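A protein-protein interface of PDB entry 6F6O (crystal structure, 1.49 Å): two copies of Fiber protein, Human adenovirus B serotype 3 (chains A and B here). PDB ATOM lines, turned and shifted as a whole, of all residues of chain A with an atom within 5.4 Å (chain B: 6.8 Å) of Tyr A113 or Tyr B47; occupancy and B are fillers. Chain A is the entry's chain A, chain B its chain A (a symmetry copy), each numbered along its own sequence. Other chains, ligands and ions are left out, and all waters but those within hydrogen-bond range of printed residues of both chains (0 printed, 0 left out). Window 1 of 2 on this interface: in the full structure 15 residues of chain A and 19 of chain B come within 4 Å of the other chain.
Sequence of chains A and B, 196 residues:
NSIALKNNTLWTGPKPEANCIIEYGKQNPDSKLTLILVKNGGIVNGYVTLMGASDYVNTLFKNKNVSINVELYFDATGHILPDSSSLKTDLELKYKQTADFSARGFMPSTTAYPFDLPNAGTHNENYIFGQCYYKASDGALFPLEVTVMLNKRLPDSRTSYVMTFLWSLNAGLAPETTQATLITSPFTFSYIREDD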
ATOM      1  N   ILE A  43      -8.118 -24.906  12.418  1.00  0.00           N
ATOM      2  CA  ILE A  43      -8.407 -23.507  12.141  1.00  0.00           C
ATOM      3  C   ILE A  43      -9.212 -23.345  10.845  1.00  0.00           C
ATOM      4  O   ILE A  43      -9.191 -24.224   9.981  1.00  0.00           O
ATOM      5  CB  ILE A  43      -7.074 -22.720  12.008  1.00  0.00           C
ATOM      6  CG1 ILE A  43      -6.248 -22.874  13.294  1.00  0.00           C
ATOM      7  CG2 ILE A  43      -7.240 -21.333  11.564  1.00  0.00           C
ATOM      8  CD1 ILE A  43      -6.698 -21.961  14.307  1.00  0.00           C
ATOM      9  N   PRO A 108     -17.141 -20.643  14.175  1.00  0.00           N
ATOM     10  CA  PRO A 108     -16.199 -20.320  15.239  1.00  0.00           C
ATOM     11  C   PRO A 108     -16.518 -21.114  16.522  1.00  0.00           C
ATOM     12  O   PRO A 108     -17.686 -21.156  16.974  1.00  0.00           O
ATOM     13  CB  PRO A 108     -16.426 -18.821  15.436  1.00  0.00           C
ATOM     14  CG  PRO A 108     -17.862 -18.570  14.970  1.00  0.00           C
ATOM     15  CD  PRO A 108     -17.976 -19.486  13.781  1.00  0.00           C
ATOM     16  N   SER A 109     -15.477 -21.713  17.136  1.00  0.00           N
ATOM     17  CA  SER A 109     -15.605 -22.521  18.310  1.00  0.00           C
ATOM     18  C   SER A 109     -16.258 -21.782  19.451  1.00  0.00           C
ATOM     19  O   SER A 109     -15.816 -20.689  19.794  1.00  0.00           O
ATOM     20  CB  SER A 109     -14.227 -22.984  18.754  1.00  0.00           C
ATOM     21  OG  SER A 109     -14.291 -23.627  20.029  1.00  0.00           O
ATOM     22  N   THR A 110     -17.285 -22.379  20.070  1.00  0.00           N
ATOM     23  CA  THR A 110     -17.910 -21.776  21.252  1.00  0.00           C
ATOM     24  C   THR A 110     -17.064 -22.091  22.511  1.00  0.00           C
ATOM     25  O   THR A 110     -17.312 -21.525  23.562  1.00  0.00           O
ATOM     26  CB  THR A 110     -19.346 -22.245  21.435  1.00  0.00           C
ATOM     27  OG1 THR A 110     -19.357 -23.667  21.466  1.00  0.00           O
ATOM     28  CG2 THR A 110     -20.244 -21.765  20.322  1.00  0.00           C
ATOM     29  N   THR A 111     -16.071 -22.988  22.414  1.00  0.00           N
ATOM     30  CA  THR A 111     -15.113 -23.204  23.534  1.00  0.00           C
ATOM     31  C   THR A 111     -14.060 -22.083  23.537  1.00  0.00           C
ATOM     32  O   THR A 111     -13.781 -21.469  24.553  1.00  0.00           O
ATOM     33  CB  THR A 111     -14.445 -24.572  23.374  1.00  0.00           C
ATOM     34  OG1 THR A 111     -15.478 -25.580  23.426  1.00  0.00           O
ATOM     35  CG2 THR A 111     -13.426 -24.800  24.471  1.00  0.00           C
ATOM     36  N   ALA A 112     -13.504 -21.774  22.362  1.00  0.00           N
ATOM     37  CA  ALA A 112     -12.503 -20.747  22.265  1.00  0.00           C
ATOM     38  C   ALA A 112     -13.131 -19.356  22.399  1.00  0.00           C
ATOM     39  O   ALA A 112     -12.537 -18.470  22.999  1.00  0.00           O
ATOM     40  CB  ALA A 112     -11.722 -20.856  20.953  1.00  0.00           C
ATOM     41  N   TYR A 113     -14.342 -19.167  21.816  1.00  0.00           N
ATOM     42  CA  TYR A 113     -14.996 -17.883  21.697  1.00  0.00           C
ATOM     43  C   TYR A 113     -16.424 -18.025  22.267  1.00  0.00           C
ATOM     44  O   TYR A 113     -17.361 -18.286  21.521  1.00  0.00           O
ATOM     45  CB  TYR A 113     -15.041 -17.460  20.221  1.00  0.00           C
ATOM     46  CG  TYR A 113     -13.743 -17.620  19.482  1.00  0.00           C
ATOM     47  CD1 TYR A 113     -12.584 -16.903  19.811  1.00  0.00           C
ATOM     48  CD2 TYR A 113     -13.653 -18.547  18.438  1.00  0.00           C
ATOM     49  CE1 TYR A 113     -11.381 -17.089  19.092  1.00  0.00           C
ATOM     50  CE2 TYR A 113     -12.494 -18.735  17.767  1.00  0.00           C
ATOM     51  CZ  TYR A 113     -11.369 -18.011  18.070  1.00  0.00           C
ATOM     52  OH  TYR A 113     -10.197 -18.247  17.389  1.00  0.00           O
ATOM     53  N   PRO A 114     -16.565 -17.971  23.598  1.00  0.00           N
ATOM     54  CA  PRO A 114     -17.882 -18.247  24.178  1.00  0.00           C
ATOM     55  C   PRO A 114     -18.929 -17.123  24.001  1.00  0.00           C
ATOM     56  O   PRO A 114     -18.578 -16.012  23.651  1.00  0.00           O
ATOM     57  CB  PRO A 114     -17.575 -18.426  25.656  1.00  0.00           C
ATOM     58  CG  PRO A 114     -16.117 -18.637  25.749  1.00  0.00           C
ATOM     59  CD  PRO A 114     -15.498 -17.942  24.613  1.00  0.00           C
ATOM     60  N   PHE A 115     -20.194 -17.387  24.332  1.00  0.00           N
ATOM     61  CA  PHE A 115     -21.175 -16.340  24.465  1.00  0.00           C
ATOM     62  C   PHE A 115     -21.214 -15.700  25.866  1.00  0.00           C
ATOM     63  O   PHE A 115     -21.043 -16.372  26.901  1.00  0.00           O
ATOM     64  CB  PHE A 115     -22.547 -16.935  24.056  1.00  0.00           C
ATOM     65  CG  PHE A 115     -22.676 -17.131  22.577  1.00  0.00           C
ATOM     66  CD1 PHE A 115     -22.943 -16.041  21.771  1.00  0.00           C
ATOM     67  CD2 PHE A 115     -22.541 -18.388  21.956  1.00  0.00           C
ATOM     68  CE1 PHE A 115     -23.082 -16.153  20.377  1.00  0.00           C
ATOM     69  CE2 PHE A 115     -22.670 -18.497  20.577  1.00  0.00           C
ATOM     70  CZ  PHE A 115     -22.920 -17.387  19.781  1.00  0.00           C
ATOM     71  N   GLU A 125     -11.936 -12.043  24.597  1.00  0.00           N
ATOM     72  CA  GLU A 125     -11.094 -12.862  23.761  1.00  0.00           C
ATOM     73  C   GLU A 125     -11.708 -13.248  22.419  1.00  0.00           C
ATOM     74  O   GLU A 125     -11.113 -14.042  21.648  1.00  0.00           O
ATOM     75  CB  GLU A 125     -10.615 -14.115  24.502  1.00  0.00           C
ATOM     76  CG  GLU A 125     -11.692 -15.134  24.812  1.00  0.00           C
ATOM     77  CD  GLU A 125     -12.367 -14.976  26.155  1.00  0.00           C
ATOM     78  OE1 GLU A 125     -12.499 -13.834  26.688  1.00  0.00           O
ATOM     79  OE2 GLU A 125     -12.784 -16.030  26.736  1.00  0.00           O
ATOM     80  N   ASN A 126     -12.852 -12.664  22.098  1.00  0.00           N
ATOM     81  CA  ASN A 126     -13.598 -13.057  20.917  1.00  0.00           C
ATOM     82  C   ASN A 126     -13.420 -12.106  19.761  1.00  0.00           C
ATOM     83  O   ASN A 126     -14.135 -12.216  18.752  1.00  0.00           O
ATOM     84  CB  ASN A 126     -15.070 -13.093  21.294  1.00  0.00           C
ATOM     85  CG  ASN A 126     -15.424 -14.223  22.263  1.00  0.00           C
ATOM     86  OD1 ASN A 126     -14.624 -14.640  23.130  1.00  0.00           O
ATOM     87  ND2 ASN A 126     -16.604 -14.790  22.069  1.00  0.00           N
ATOM     88  N   LEU A 150     -16.438 -12.788  17.030  1.00  0.00           N
ATOM     89  CA  LEU A 150     -16.834 -14.180  16.921  1.00  0.00           C
ATOM     90  C   LEU A 150     -17.704 -14.508  18.133  1.00  0.00           C
ATOM     91  O   LEU A 150     -17.312 -14.275  19.297  1.00  0.00           O
ATOM     92  CB  LEU A 150     -15.614 -15.122  16.885  1.00  0.00           C
ATOM     93  CG  LEU A 150     -14.668 -14.878  15.723  1.00  0.00           C
ATOM     94  CD1 LEU A 150     -13.425 -15.728  15.849  1.00  0.00           C
ATOM     95  CD2 LEU A 150     -15.362 -15.017  14.352  1.00  0.00           C
ATOM     96  N   ASN A 151     -18.902 -15.063  17.899  1.00  0.00           N
ATOM     97  CA  ASN A 151     -19.799 -15.427  18.988  1.00  0.00           C
ATOM     98  C   ASN A 151     -20.050 -14.242  19.907  1.00  0.00           C
ATOM     99  O   ASN A 151     -20.414 -13.178  19.418  1.00  0.00           O
ATOM    100  CB  ASN A 151     -19.408 -16.744  19.645  1.00  0.00           C
ATOM    101  CG  ASN A 151     -19.374 -17.860  18.624  1.00  0.00           C
ATOM    102  OD1 ASN A 151     -20.162 -17.839  17.664  1.00  0.00           O
ATOM    103  ND2 ASN A 151     -18.448 -18.821  18.788  1.00  0.00           N
ATOM    104  N   LYS A 152     -19.854 -14.375  21.211  1.00  0.00           N
ATOM    105  CA  LYS A 152     -19.948 -13.258  22.191  1.00  0.00           C
ATOM    106  C   LYS A 152     -21.390 -12.767  22.467  1.00  0.00           C
ATOM    107  O   LYS A 152     -21.926 -12.922  23.573  1.00  0.00           O
ATOM    108  CB  LYS A 152     -19.001 -12.088  21.931  1.00  0.00           C
ATOM    109  CG  LYS A 152     -18.998 -11.082  23.091  1.00  0.00           C
ATOM    110  CD  LYS A 152     -17.973  -9.950  22.870  1.00  0.00           C
ATOM    111  CE  LYS A 152     -18.074  -8.794  23.882  1.00  0.00           C
ATOM    112  NZ  LYS A 152     -17.992  -9.252  25.249  1.00  0.00           N
ATOM    113  N   SER A 190      -7.838 -15.691  10.737  1.00  0.00           N
ATOM    114  CA  SER A 190      -7.906 -17.121  11.095  1.00  0.00           C
ATOM    115  C   SER A 190      -8.522 -17.262  12.463  1.00  0.00           C
ATOM    116  O   SER A 190      -8.339 -16.432  13.372  1.00  0.00           O
ATOM    117  CB  SER A 190      -6.546 -17.756  11.130  1.00  0.00           C
ATOM    118  OG  SER A 190      -5.941 -17.725   9.843  1.00  0.00           O
ATOM    119  N   TYR A 191      -9.293 -18.313  12.637  1.00  0.00           N
ATOM    120  CA  TYR A 191      -9.920 -18.595  13.915  1.00  0.00           C
ATOM    121  C   TYR A 191     -10.065 -20.103  14.209  1.00  0.00           C
ATOM    122  O   TYR A 191     -10.044 -20.947  13.309  1.00  0.00           O
ATOM    123  CB  TYR A 191     -11.270 -17.850  14.029  1.00  0.00           C
ATOM    124  CG  TYR A 191     -12.323 -18.320  13.027  1.00  0.00           C
ATOM    125  CD1 TYR A 191     -13.139 -19.414  13.268  1.00  0.00           C
ATOM    126  CD2 TYR A 191     -12.493 -17.621  11.862  1.00  0.00           C
ATOM    127  CE1 TYR A 191     -14.088 -19.831  12.336  1.00  0.00           C
ATOM    128  CE2 TYR A 191     -13.449 -18.007  10.946  1.00  0.00           C
ATOM    129  CZ  TYR A 191     -14.242 -19.082  11.195  1.00  0.00           C
ATOM    130  OH  TYR A 191     -15.175 -19.455  10.251  1.00  0.00           O
ATOM    131  N   ILE A 192     -10.208 -20.475  15.471  1.00  0.00           N
ATOM    132  CA  ILE A 192     -10.360 -21.840  15.942  1.00  0.00           C
ATOM    133  C   ILE A 192     -11.791 -22.287  15.645  1.00  0.00           C
ATOM    134  O   ILE A 192     -12.745 -21.620  15.976  1.00  0.00           O
ATOM    135  CB  ILE A 192     -10.106 -21.918  17.471  1.00  0.00           C
ATOM    136  CG1 ILE A 192      -8.669 -21.465  17.764  1.00  0.00           C
ATOM    137  CG2 ILE A 192     -10.406 -23.296  17.950  1.00  0.00           C
ATOM    138  CD1 ILE A 192      -8.426 -21.163  19.253  1.00  0.00           C
ATOM    139  N   PRO B  14      -7.555 -25.610  22.481  1.00  0.00           N
ATOM    140  CA  PRO B  14      -8.178 -24.347  22.068  1.00  0.00           C
ATOM    141  C   PRO B  14      -8.462 -23.353  23.173  1.00  0.00           C
ATOM    142  O   PRO B  14      -8.720 -22.205  22.862  1.00  0.00           O
ATOM    143  CB  PRO B  14      -9.527 -24.850  21.501  1.00  0.00           C
ATOM    144  CG  PRO B  14      -9.876 -26.017  22.366  1.00  0.00           C
ATOM    145  CD  PRO B  14      -8.539 -26.704  22.452  1.00  0.00           C
ATOM    146  N   LYS B  15      -8.482 -23.797  24.435  1.00  0.00           N
ATOM    147  CA  LYS B  15      -8.800 -22.903  25.577  1.00  0.00           C
ATOM    148  C   LYS B  15      -8.068 -23.420  26.845  1.00  0.00           C
ATOM    149  O   LYS B  15      -8.667 -23.891  27.822  1.00  0.00           O
ATOM    150  CB  LYS B  15     -10.355 -22.763  25.800  1.00  0.00           C
ATOM    151  CG  LYS B  15     -10.775 -21.490  26.528  1.00  0.00           C
ATOM    152  CD  LYS B  15     -10.356 -20.252  25.741  1.00  0.00           C
ATOM    153  CE  LYS B  15     -10.720 -18.920  26.407  1.00  0.00           C
ATOM    154  NZ  LYS B  15     -12.015 -18.455  25.937  1.00  0.00           N
ATOM    155  N   THR B  34      -2.250 -19.784  24.134  1.00  0.00           N
ATOM    156  CA  THR B  34      -2.842 -20.561  23.071  1.00  0.00           C
ATOM    157  C   THR B  34      -1.922 -20.494  21.876  1.00  0.00           C
ATOM    158  O   THR B  34      -1.640 -19.425  21.373  1.00  0.00           O
ATOM    159  CB  THR B  34      -4.238 -20.066  22.698  1.00  0.00           C
ATOM    160  OG1 THR B  34      -5.108 -20.133  23.822  1.00  0.00           O
ATOM    161  CG2 THR B  34      -4.801 -20.945  21.635  1.00  0.00           C
ATOM    162  N   LEU B  35      -1.396 -21.644  21.452  1.00  0.00           N
ATOM    163  CA  LEU B  35      -0.522 -21.707  20.284  1.00  0.00           C
ATOM    164  C   LEU B  35      -0.970 -22.849  19.409  1.00  0.00           C
ATOM    165  O   LEU B  35      -1.142 -24.000  19.891  1.00  0.00           O
ATOM    166  CB  LEU B  35       0.959 -21.895  20.641  1.00  0.00           C
ATOM    167  CG  LEU B  35       1.917 -22.009  19.472  1.00  0.00           C
ATOM    168  CD1 LEU B  35       2.014 -20.746  18.669  1.00  0.00           C
ATOM    169  CD2 LEU B  35       3.297 -22.449  19.972  1.00  0.00           C
ATOM    170  N   ILE B  36      -1.201 -22.562  18.119  1.00  0.00           N
ATOM    171  CA  ILE B  36      -1.708 -23.552  17.185  1.00  0.00           C
ATOM    172  C   ILE B  36      -0.863 -23.522  15.937  1.00  0.00           C
ATOM    173  O   ILE B  36      -0.707 -22.430  15.357  1.00  0.00           O
ATOM    174  CB  ILE B  36      -3.201 -23.304  16.821  1.00  0.00           C
ATOM    175  CG1 ILE B  36      -4.013 -23.179  18.131  1.00  0.00           C
ATOM    176  CG2 ILE B  36      -3.730 -24.351  15.875  1.00  0.00           C
ATOM    177  CD1 ILE B  36      -5.468 -22.828  17.890  1.00  0.00           C
ATOM    178  N   LEU B  37      -0.306 -24.643  15.514  1.00  0.00           N
ATOM    179  CA  LEU B  37       0.577 -24.767  14.337  1.00  0.00           C
ATOM    180  C   LEU B  37      -0.052 -25.764  13.412  1.00  0.00           C
ATOM    181  O   LEU B  37      -0.263 -26.897  13.795  1.00  0.00           O
ATOM    182  CB  LEU B  37       1.972 -25.211  14.730  1.00  0.00           C
ATOM    183  CG  LEU B  37       2.715 -24.394  15.820  1.00  0.00           C
ATOM    184  CD1 LEU B  37       4.013 -25.044  16.247  1.00  0.00           C
ATOM    185  CD2 LEU B  37       2.947 -22.952  15.357  1.00  0.00           C
ATOM    186  N   VAL B  38      -0.435 -25.360  12.198  1.00  0.00           N
ATOM    187  CA  VAL B  38      -1.052 -26.217  11.227  1.00  0.00           C
ATOM    188  C   VAL B  38      -0.141 -26.335   9.992  1.00  0.00           C
ATOM    189  O   VAL B  38       0.268 -25.309   9.390  1.00  0.00           O
ATOM    190  CB  VAL B  38      -2.398 -25.708  10.785  1.00  0.00           C
ATOM    191  CG1 VAL B  38      -3.001 -26.603   9.765  1.00  0.00           C
ATOM    192  CG2 VAL B  38      -3.300 -25.507  11.991  1.00  0.00           C
ATOM    193  N   ASN B  45       1.148 -22.590   9.213  1.00  0.00           N
ATOM    194  CA  ASN B  45       0.301 -21.463   9.582  1.00  0.00           C
ATOM    195  C   ASN B  45       0.126 -21.497  11.113  1.00  0.00           C
ATOM    196  O   ASN B  45      -0.390 -22.484  11.678  1.00  0.00           O
ATOM    197  CB  ASN B  45      -1.045 -21.585   8.879  1.00  0.00           C
ATOM    198  CG  ASN B  45      -0.966 -21.419   7.394  1.00  0.00           C
ATOM    199  OD1 ASN B  45      -1.643 -22.167   6.673  1.00  0.00           O
ATOM    200  ND2 ASN B  45      -0.180 -20.479   6.911  1.00  0.00           N
ATOM    201  N   GLY B  46       0.536 -20.430  11.784  1.00  0.00           N
ATOM    202  CA  GLY B  46       0.463 -20.302  13.223  1.00  0.00           C
ATOM    203  C   GLY B  46      -0.557 -19.311  13.663  1.00  0.00           C
ATOM    204  O   GLY B  46      -0.885 -18.314  12.954  1.00  0.00           O
ATOM    205  N   TYR B  47      -1.030 -19.539  14.904  1.00  0.00           N
ATOM    206  CA  TYR B  47      -2.009 -18.692  15.569  1.00  0.00           C
ATOM    207  C   TYR B  47      -1.607 -18.621  17.032  1.00  0.00           C
ATOM    208  O   TYR B  47      -1.364 -19.671  17.649  1.00  0.00           O
ATOM    209  CB  TYR B  47      -3.406 -19.315  15.437  1.00  0.00           C
ATOM    210  CG  TYR B  47      -4.547 -18.747  16.263  1.00  0.00           C
ATOM    211  CD1 TYR B  47      -4.655 -19.005  17.606  1.00  0.00           C
ATOM    212  CD2 TYR B  47      -5.599 -18.077  15.654  1.00  0.00           C
ATOM    213  CE1 TYR B  47      -5.750 -18.573  18.343  1.00  0.00           C
ATOM    214  CE2 TYR B  47      -6.685 -17.648  16.355  1.00  0.00           C
ATOM    215  CZ  TYR B  47      -6.813 -17.897  17.725  1.00  0.00           C
ATOM    216  OH  TYR B  47      -7.914 -17.432  18.454  1.00  0.00           O
ATOM    217  N   VAL B  48      -1.501 -17.447  17.624  1.00  0.00           N
ATOM    218  CA  VAL B  48      -1.041 -17.303  19.006  1.00  0.00           C
ATOM    219  C   VAL B  48      -1.798 -16.183  19.782  1.00  0.00           C
ATOM    220  O   VAL B  48      -2.069 -15.125  19.202  1.00  0.00           O
ATOM    221  CB  VAL B  48       0.493 -17.092  19.083  1.00  0.00           C
ATOM    222  CG1 VAL B  48       0.920 -15.777  18.461  1.00  0.00           C
ATOM    223  CG2 VAL B  48       0.992 -17.204  20.530  1.00  0.00           C
ATOM    224  N   THR B  49      -2.202 -16.462  21.014  1.00  0.00           N
ATOM    225  CA  THR B  49      -2.769 -15.484  21.909  1.00  0.00           C
ATOM    226  C   THR B  49      -2.374 -15.819  23.328  1.00  0.00           C
ATOM    227  O   THR B  49      -2.179 -16.992  23.674  1.00  0.00           O
ATOM    228  CB  THR B  49      -4.320 -15.305  21.766  1.00  0.00           C
ATOM    229  OG1 THR B  49      -4.855 -14.464  22.834  1.00  0.00           O
ATOM    230  CG2 THR B  49      -5.106 -16.641  21.740  1.00  0.00           C
ATOM    231  N   PHE B 165       8.416 -15.198  21.119  1.00  0.00           N
ATOM    232  CA  PHE B 165       7.389 -14.153  20.900  1.00  0.00           C
ATOM    233  C   PHE B 165       7.644 -12.999  21.797  1.00  0.00           C
ATOM    234  O   PHE B 165       7.891 -13.177  23.016  1.00  0.00           O
ATOM    235  CB  PHE B 165       5.979 -14.690  21.194  1.00  0.00           C
ATOM    236  CG  PHE B 165       5.587 -15.868  20.338  1.00  0.00           C
ATOM    237  CD1 PHE B 165       5.014 -15.651  19.121  1.00  0.00           C
ATOM    238  CD2 PHE B 165       5.779 -17.159  20.758  1.00  0.00           C
ATOM    239  CE1 PHE B 165       4.681 -16.701  18.302  1.00  0.00           C
ATOM    240  CE2 PHE B 165       5.426 -18.211  19.941  1.00  0.00           C
ATOM    241  CZ  PHE B 165       4.882 -17.986  18.721  1.00  0.00           C
ATOM    242  N   SER B 185      -4.986  -9.941  21.337  1.00  0.00           N
ATOM    243  CA  SER B 185      -5.860 -10.435  20.246  1.00  0.00           C
ATOM    244  C   SER B 185      -5.055 -11.378  19.367  1.00  0.00           C
ATOM    245  O   SER B 185      -3.821 -11.266  19.296  1.00  0.00           O
ATOM    246  CB  SER B 185      -6.465  -9.244  19.463  1.00  0.00           C
ATOM    247  OG  SER B 185      -5.511  -8.602  18.648  1.00  0.00           O
ATOM    248  N   PRO B 186      -5.699 -12.332  18.731  1.00  0.00           N
ATOM    249  CA  PRO B 186      -4.912 -13.367  18.055  1.00  0.00           C
ATOM    250  C   PRO B 186      -4.036 -12.853  16.949  1.00  0.00           C
ATOM    251  O   PRO B 186      -4.427 -11.971  16.147  1.00  0.00           O
ATOM    252  CB  PRO B 186      -5.963 -14.324  17.527  1.00  0.00           C
ATOM    253  CG  PRO B 186      -7.192 -14.018  18.258  1.00  0.00           C
ATOM    254  CD  PRO B 186      -7.142 -12.625  18.725  1.00  0.00           C
ATOM    255  N   PHE B 187      -2.828 -13.396  16.894  1.00  0.00           N
ATOM    256  CA  PHE B 187      -1.798 -13.017  15.954  1.00  0.00           C
ATOM    257  C   PHE B 187      -1.528 -14.235  15.061  1.00  0.00           C
ATOM    258  O   PHE B 187      -1.306 -15.319  15.574  1.00  0.00           O
ATOM    259  CB  PHE B 187      -0.500 -12.556  16.627  1.00  0.00           C
ATOM    260  CG  PHE B 187       0.572 -12.164  15.677  1.00  0.00           C
ATOM    261  CD1 PHE B 187       0.437 -11.065  14.876  1.00  0.00           C
ATOM    262  CD2 PHE B 187       1.713 -12.978  15.500  1.00  0.00           C
ATOM    263  CE1 PHE B 187       1.394 -10.709  13.937  1.00  0.00           C
ATOM    264  CE2 PHE B 187       2.691 -12.578  14.585  1.00  0.00           C
ATOM    265  CZ  PHE B 187       2.496 -11.481  13.765  1.00  0.00           C
ATOM    266  N   THR B 188      -1.564 -14.026  13.764  1.00  0.00           N
ATOM    267  CA  THR B 188      -1.328 -15.087  12.785  1.00  0.00           C
ATOM    268  C   THR B 188      -0.054 -14.816  12.074  1.00  0.00           C
ATOM    269  O   THR B 188       0.332 -13.649  11.791  1.00  0.00           O
ATOM    270  CB  THR B 188      -2.473 -15.261  11.826  1.00  0.00           C
ATOM    271  OG1 THR B 188      -2.725 -14.026  11.157  1.00  0.00           O
ATOM    272  CG2 THR B 188      -3.730 -15.753  12.520  1.00  0.00           C
ATOM    273  N   PHE B 189       0.654 -15.916  11.730  1.00  0.00           N
ATOM    274  CA  PHE B 189       1.927 -15.857  11.094  1.00  0.00           C
ATOM    275  C   PHE B 189       2.164 -17.159  10.352  1.00  0.00           C
ATOM    276  O   PHE B 189       1.474 -18.140  10.601  1.00  0.00           O
ATOM    277  CB  PHE B 189       3.026 -15.580  12.067  1.00  0.00           C
ATOM    278  CG  PHE B 189       3.177 -16.608  13.178  1.00  0.00           C
ATOM    279  CD1 PHE B 189       2.317 -16.687  14.265  1.00  0.00           C
ATOM    280  CD2 PHE B 189       4.181 -17.535  13.108  1.00  0.00           C
ATOM    281  CE1 PHE B 189       2.484 -17.611  15.271  1.00  0.00           C
ATOM    282  CE2 PHE B 189       4.357 -18.449  14.122  1.00  0.00           C
ATOM    283  CZ  PHE B 189       3.491 -18.554  15.175  1.00  0.00           C
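NZ of Lys B15 lies within salt-bridge range of OE2 of Glu A125 (2.7 Å).
NZ of Lys B15 sits at hydrogen-bond distance from O of Ala A112, 3.0 Å away.
The side-chain hydroxyl (OH) of Tyr A113 sits at hydrogen-bond distance from the side-chain hydroxyl (OH) of Tyr B47 (2.6 Å).
The backbone carbonyl oxygen (O) of Tyr A113 sits at hydrogen-bond distance from the side-chain amide nitrogen (ND2) of Asn A151 (3.0 Å).
O of Pro A114 lies within hydrogen-bond range of N of Lys A152 (3.2 Å).
N of Ser A109 lies within hydrogen-bond range of O of Ile A192, 3.0 Å away.
The backbone NH of Ala A112 sits at hydrogen-bond distance from the side-chain hydroxyl of Ser A109 (3.1 Å).
The backbone NH (N) of Ile B36 lies within hydrogen-bond range of the backbone carbonyl oxygen (O) of Tyr B47 (2.9 Å).
ND2 of Asn A126 sits at hydrogen-bond distance from O of Pro A114 (2.8 Å).
Ile A43 touches Ile B36 (CD1 to CD1, 3.9 Å).
Thr A111 touches Lys B15.
Pro B14 touches Ala A112.
CD of Pro A114 touches NZ of Lys B15, at 3.8 Å.
Ser A190 touches Tyr B47.
Ser A190 touches Thr B188.
Pro B14 touches Ile A192 (O to CD1, 3.8 Å).
Ile B36 touches Ile A192 (CD1 to CG1, 3.5 Å).
Ile A192 touches Tyr B47 (CD1 to CE1, 3.8 Å).
Of the printed residues of chain B, Tyr A113 touches Tyr B47 (2.6 Å).
Tyr B47 touches just these residues of chain A: Tyr A113, Ser A190 and Ile A192.
Of the printed residues of chain A, Pro B14 touches Ala A112 and Ile A192.
Of the printed residues of chain B, Thr A111 touches Lys B15 (3.6 Å).
Of the printed residues of chain B, Ser A190 touches Tyr B47 and Thr B188.
Phe B189 touches none of the printed residues of chain A.
The nearest residue of chain B that does not touch Tyr A113 is Lys B15 (4.8 Å).
Of the 17 printed residues of chain A, 8 touch a printed residue of chain B.
Of the 18 printed residues of chain B, 5 touch a printed residue of chain A.
Hydrophobic or aromatic side chains of chain B within 4 Å of the printed part of chain A: Pro B14, Ile B36 and Tyr B47.
Among the printed residues, 12 pairs touch across the chains.
Among the printed residues, Asp or Glu carboxylates within 4 Å of a Lys or Arg side-chain nitrogen of the other chain: Glu A125 with Lys B15 (2.7 Å).
No position is printed for both chains.
Of the 12 pairs that touch across the chains among the printed residues, none has its exchanged pair printed and touching as well.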
